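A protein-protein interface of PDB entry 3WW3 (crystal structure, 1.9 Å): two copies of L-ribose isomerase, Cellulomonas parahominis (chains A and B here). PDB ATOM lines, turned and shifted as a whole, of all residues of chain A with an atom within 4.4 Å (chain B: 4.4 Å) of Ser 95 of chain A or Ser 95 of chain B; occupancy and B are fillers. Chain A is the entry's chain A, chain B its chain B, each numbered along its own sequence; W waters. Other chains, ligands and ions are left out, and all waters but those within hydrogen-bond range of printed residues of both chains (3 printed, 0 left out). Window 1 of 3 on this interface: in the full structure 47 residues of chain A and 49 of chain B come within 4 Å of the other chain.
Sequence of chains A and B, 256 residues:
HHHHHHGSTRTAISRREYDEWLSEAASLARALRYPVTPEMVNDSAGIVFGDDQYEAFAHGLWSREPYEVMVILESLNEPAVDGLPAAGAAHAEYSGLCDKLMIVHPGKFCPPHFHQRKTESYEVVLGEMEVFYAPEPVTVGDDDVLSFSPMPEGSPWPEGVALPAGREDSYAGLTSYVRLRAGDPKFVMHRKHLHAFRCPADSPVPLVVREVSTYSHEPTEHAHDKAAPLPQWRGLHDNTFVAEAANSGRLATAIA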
ATOM      1  N   HIS A  91      19.535  22.430  32.248  1.00  0.00           N
ATOM      2  CA  HIS A  91      19.914  21.851  30.967  1.00  0.00           C
ATOM      3  C   HIS A  91      19.591  22.730  29.768  1.00  0.00           C
ATOM      4  O   HIS A  91      19.606  22.262  28.632  1.00  0.00           O
ATOM      5  CB  HIS A  91      19.260  20.481  30.798  1.00  0.00           C
ATOM      6  CG  HIS A  91      19.606  19.515  31.888  1.00  0.00           C
ATOM      7  ND1 HIS A  91      18.985  19.528  33.119  1.00  0.00           N
ATOM      8  CD2 HIS A  91      20.545  18.541  31.950  1.00  0.00           C
ATOM      9  CE1 HIS A  91      19.529  18.605  33.893  1.00  0.00           C
ATOM     10  NE2 HIS A  91      20.477  17.992  33.207  1.00  0.00           N
ATOM     11  N   ALA A  92      19.307  24.005  30.019  1.00  0.00           N
ATOM     12  CA  ALA A  92      18.999  24.935  28.939  1.00  0.00           C
ATOM     13  C   ALA A  92      20.202  25.044  28.011  1.00  0.00           C
ATOM     14  O   ALA A  92      20.058  25.345  26.823  1.00  0.00           O
ATOM     15  CB  ALA A  92      18.654  26.306  29.507  1.00  0.00           C
ATOM     16  N   GLU A  93      21.387  24.787  28.562  1.00  0.00           N
ATOM     17  CA  GLU A  93      22.632  24.862  27.805  1.00  0.00           C
ATOM     18  C   GLU A  93      22.742  23.791  26.716  1.00  0.00           C
ATOM     19  O   GLU A  93      23.618  23.872  25.853  1.00  0.00           O
ATOM     20  CB  GLU A  93      23.826  24.767  28.756  1.00  0.00           C
ATOM     21  CG  GLU A  93      23.947  23.443  29.476  1.00  0.00           C
ATOM     22  CD  GLU A  93      24.781  23.555  30.737  1.00  0.00           C
ATOM     23  OE1 GLU A  93      24.349  24.271  31.665  1.00  0.00           O
ATOM     24  OE2 GLU A  93      25.866  22.938  30.799  1.00  0.00           O
ATOM     25  N   TYR A  94      21.868  22.790  26.759  1.00  0.00           N
ATOM     26  CA  TYR A  94      21.875  21.743  25.736  1.00  0.00           C
ATOM     27  C   TYR A  94      20.930  22.128  24.602  1.00  0.00           C
ATOM     28  O   TYR A  94      20.837  21.435  23.585  1.00  0.00           O
ATOM     29  CB  TYR A  94      21.442  20.397  26.322  1.00  0.00           C
ATOM     30  CG  TYR A  94      22.445  19.813  27.284  1.00  0.00           C
ATOM     31  CD1 TYR A  94      22.529  20.270  28.599  1.00  0.00           C
ATOM     32  CD2 TYR A  94      23.349  18.837  26.865  1.00  0.00           C
ATOM     33  CE1 TYR A  94      23.492  19.770  29.474  1.00  0.00           C
ATOM     34  CE2 TYR A  94      24.314  18.335  27.726  1.00  0.00           C
ATOM     35  CZ  TYR A  94      24.381  18.806  29.030  1.00  0.00           C
ATOM     36  OH  TYR A  94      25.347  18.319  29.879  1.00  0.00           O
ATOM     37  N   SER A  95      20.232  23.242  24.780  1.00  0.00           N
ATOM     38  CA  SER A  95      19.284  23.714  23.780  1.00  0.00           C
ATOM     39  C   SER A  95      19.778  24.976  23.082  1.00  0.00           C
ATOM     40  O   SER A  95      20.982  25.188  22.946  1.00  0.00           O
ATOM     41  CB  SER A  95      17.919  23.962  24.434  1.00  0.00           C
ATOM     42  OG  SER A  95      16.942  24.319  23.465  1.00  0.00           O
ATOM     43  N   GLY A  96      18.848  25.812  22.628  1.00  0.00           N
ATOM     44  CA  GLY A  96      19.235  27.026  21.938  1.00  0.00           C
ATOM     45  C   GLY A  96      19.288  26.792  20.437  1.00  0.00           C
ATOM     46  O   GLY A  96      19.126  25.657  19.976  1.00  0.00           O
ATOM     47  N   THR A 214      22.337  23.365  18.145  1.00  0.00           N
ATOM     48  CA  THR A 214      21.865  23.965  19.383  1.00  0.00           C
ATOM     49  C   THR A 214      22.883  25.066  19.681  1.00  0.00           C
ATOM     50  O   THR A 214      23.814  25.275  18.894  1.00  0.00           O
ATOM     51  CB  THR A 214      21.774  22.934  20.544  1.00  0.00           C
ATOM     52  OG1 THR A 214      23.012  22.226  20.677  1.00  0.00           O
ATOM     53  CG2 THR A 214      20.647  21.941  20.275  1.00  0.00           C
ATOM     54  N   TYR A 215      22.715  25.768  20.799  1.00  0.00           N
ATOM     55  CA  TYR A 215      23.599  26.877  21.152  1.00  0.00           C
ATOM     56  C   TYR A 215      25.094  26.579  21.084  1.00  0.00           C
ATOM     57  O   TYR A 215      25.551  25.515  21.495  1.00  0.00           O
ATOM     58  CB  TYR A 215      23.262  27.393  22.555  1.00  0.00           C
ATOM     59  CG  TYR A 215      23.861  28.749  22.865  1.00  0.00           C
ATOM     60  CD1 TYR A 215      23.286  29.920  22.367  1.00  0.00           C
ATOM     61  CD2 TYR A 215      24.994  28.866  23.672  1.00  0.00           C
ATOM     62  CE1 TYR A 215      23.823  31.175  22.670  1.00  0.00           C
ATOM     63  CE2 TYR A 215      25.539  30.113  23.979  1.00  0.00           C
ATOM     64  CZ  TYR A 215      24.948  31.262  23.477  1.00  0.00           C
ATOM     65  OH  TYR A 215      25.466  32.498  23.803  1.00  0.00           O
ATOM     66  N   HIS B  91      12.387  18.833  30.136  1.00  0.00           N
ATOM     67  CA  HIS B  91      12.342  20.021  29.295  1.00  0.00           C
ATOM     68  C   HIS B  91      13.006  19.869  27.932  1.00  0.00           C
ATOM     69  O   HIS B  91      13.316  20.861  27.272  1.00  0.00           O
ATOM     70  CB  HIS B  91      12.963  21.190  30.057  1.00  0.00           C
ATOM     71  CG  HIS B  91      12.300  21.459  31.372  1.00  0.00           C
ATOM     72  ND1 HIS B  91      11.118  22.162  31.481  1.00  0.00           N
ATOM     73  CD2 HIS B  91      12.624  21.072  32.628  1.00  0.00           C
ATOM     74  CE1 HIS B  91      10.744  22.197  32.747  1.00  0.00           C
ATOM     75  NE2 HIS B  91      11.639  21.542  33.465  1.00  0.00           N
ATOM     76  N   ALA B  92      13.217  18.629  27.509  1.00  0.00           N
ATOM     77  CA  ALA B  92      13.831  18.377  26.210  1.00  0.00           C
ATOM     78  C   ALA B  92      12.892  18.856  25.106  1.00  0.00           C
ATOM     79  O   ALA B  92      13.334  19.230  24.020  1.00  0.00           O
ATOM     80  CB  ALA B  92      14.117  16.886  26.047  1.00  0.00           C
ATOM     81  N   GLU B  93      11.593  18.853  25.401  1.00  0.00           N
ATOM     82  CA  GLU B  93      10.571  19.267  24.443  1.00  0.00           C
ATOM     83  C   GLU B  93      10.652  20.737  24.044  1.00  0.00           C
ATOM     84  O   GLU B  93      10.034  21.149  23.057  1.00  0.00           O
ATOM     85  CB  GLU B  93       9.185  18.966  25.007  1.00  0.00           C
ATOM     86  CG  GLU B  93       8.866  19.732  26.274  1.00  0.00           C
ATOM     87  CD  GLU B  93       7.773  19.065  27.076  1.00  0.00           C
ATOM     88  OE1 GLU B  93       8.011  17.939  27.558  1.00  0.00           O
ATOM     89  OE2 GLU B  93       6.683  19.660  27.217  1.00  0.00           O
ATOM     90  N   TYR B  94      11.388  21.530  24.818  1.00  0.00           N
ATOM     91  CA  TYR B  94      11.554  22.944  24.499  1.00  0.00           C
ATOM     92  C   TYR B  94      12.801  23.101  23.635  1.00  0.00           C
ATOM     93  O   TYR B  94      13.123  24.198  23.186  1.00  0.00           O
ATOM     94  CB  TYR B  94      11.716  23.785  25.769  1.00  0.00           C
ATOM     95  CG  TYR B  94      10.495  23.806  26.658  1.00  0.00           C
ATOM     96  CD1 TYR B  94      10.197  22.732  27.495  1.00  0.00           C
ATOM     97  CD2 TYR B  94       9.629  24.900  26.653  1.00  0.00           C
ATOM     98  CE1 TYR B  94       9.062  22.748  28.308  1.00  0.00           C
ATOM     99  CE2 TYR B  94       8.493  24.923  27.461  1.00  0.00           C
ATOM    100  CZ  TYR B  94       8.217  23.844  28.283  1.00  0.00           C
ATOM    101  OH  TYR B  94       7.084  23.861  29.066  1.00  0.00           O
ATOM    102  N   SER B  95      13.497  21.994  23.404  1.00  0.00           N
ATOM    103  CA  SER B  95      14.717  22.021  22.608  1.00  0.00           C
ATOM    104  C   SER B  95      14.506  21.353  21.255  1.00  0.00           C
ATOM    105  O   SER B  95      13.398  21.359  20.721  1.00  0.00           O
ATOM    106  CB  SER B  95      15.847  21.325  23.377  1.00  0.00           C
ATOM    107  OG  SER B  95      17.088  21.472  22.710  1.00  0.00           O
ATOM    108  N   GLY B  96      15.568  20.773  20.704  1.00  0.00           N
ATOM    109  CA  GLY B  96      15.462  20.128  19.408  1.00  0.00           C
ATOM    110  C   GLY B  96      15.796  21.108  18.299  1.00  0.00           C
ATOM    111  O   GLY B  96      16.045  22.285  18.561  1.00  0.00           O
ATOM    112  N   THR B 214      13.120  25.383  17.389  1.00  0.00           N
ATOM    113  CA  THR B 214      13.308  24.215  18.228  1.00  0.00           C
ATOM    114  C   THR B 214      12.321  23.179  17.671  1.00  0.00           C
ATOM    115  O   THR B 214      11.580  23.474  16.730  1.00  0.00           O
ATOM    116  CB  THR B 214      13.039  24.522  19.725  1.00  0.00           C
ATOM    117  OG1 THR B 214      11.747  25.120  19.890  1.00  0.00           O
ATOM    118  CG2 THR B 214      14.106  25.477  20.255  1.00  0.00           C
ATOM    119  N   TYR B 215      12.313  21.976  18.232  1.00  0.00           N
ATOM    120  CA  TYR B 215      11.453  20.903  17.734  1.00  0.00           C
ATOM    121  C   TYR B 215       9.986  21.280  17.494  1.00  0.00           C
ATOM    122  O   TYR B 215       9.376  21.978  18.298  1.00  0.00           O
ATOM    123  CB  TYR B 215      11.520  19.713  18.687  1.00  0.00           C
ATOM    124  CG  TYR B 215      10.947  18.438  18.121  1.00  0.00           C
ATOM    125  CD1 TYR B 215      11.674  17.655  17.219  1.00  0.00           C
ATOM    126  CD2 TYR B 215       9.684  17.995  18.508  1.00  0.00           C
ATOM    127  CE1 TYR B 215      11.153  16.458  16.722  1.00  0.00           C
ATOM    128  CE2 TYR B 215       9.157  16.804  18.020  1.00  0.00           C
ATOM    129  CZ  TYR B 215       9.895  16.040  17.131  1.00  0.00           C
ATOM    130  OH  TYR B 215       9.366  14.859  16.665  1.00  0.00           O
HETATM  131  O   HOH W   1      18.387  19.210  23.811  1.00  0.00           O
HETATM  132  O   HOH W   2      17.323  23.624  20.693  1.00  0.00           O
HETATM  133  O   HOH W   3      15.241  25.687  25.428  1.00  0.00           O
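Water W2 lies within hydrogen-bond range of the backbone carbonyl oxygen (O) of Gly 96 of chain A, the backbone carbonyl oxygen (O) of Gly 96 of chain B, the side-chain hydroxyl (OG) of Ser 95 of chain A and the side-chain hydroxyl (OG) of Ser 95 of chain B. Water W1 bridges OG of Ser 95 of chain B (2.8 Å) and O of Tyr 94 of chain A (3.3 Å). Water W3 bridges OG of Ser 95 of chain A and O of Tyr 94 of chain B.
Tyr 94 of chain A touches Ser 95 of chain B (O to OG, 3.8 Å). Tyr 94 of chain B touches Ser 95 of chain A.
N of Tyr 215 of chain A lies within hydrogen-bond range of O of Ser 95 of chain A (2.8 Å). N of Tyr 215 of chain B lies within hydrogen-bond range of O of Ser 95 of chain B.
Tyr 94 of chain A touches Ser 95 of chain B, and with the chains exchanged Ser 95 of chain A touches Tyr 94 of chain B. Ser 95 of chain B touches its own counterpart, Ser 95 of chain A. Positions printed for both chains: 91, 92, 93, 94, 95, 96, 214 and 215. Of the 3 pairs that touch across the chains among the printed residues, 3 have their exchanged pair printed and touching as well.
The side-chain hydroxyl (OG) of Ser 95 of chain B is in hydrogen-bond range of the side-chain hydroxyl (OG) of Ser 95 of chain A (2.9 Å).
Of the 8 printed residues of chain B, 2 touch a printed residue of chain A. Among the printed residues, 3 pairs touch across the chains.
Of the printed residues of chain B, Ser 95 of chain A touches Tyr 94 and Ser 95. Of chain A, only Tyr 94 and Ser 95 come within 4 Å of Ser 95 of chain B. Of the printed residues of chain A, Tyr 94 of chain B touches Ser 95 (3.8 Å). Of the printed residues of chain B, Tyr 94 of chain A touches Ser 95 (3.8 Å). Tyr 215 of chain A touches none of the printed residues of chain B.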
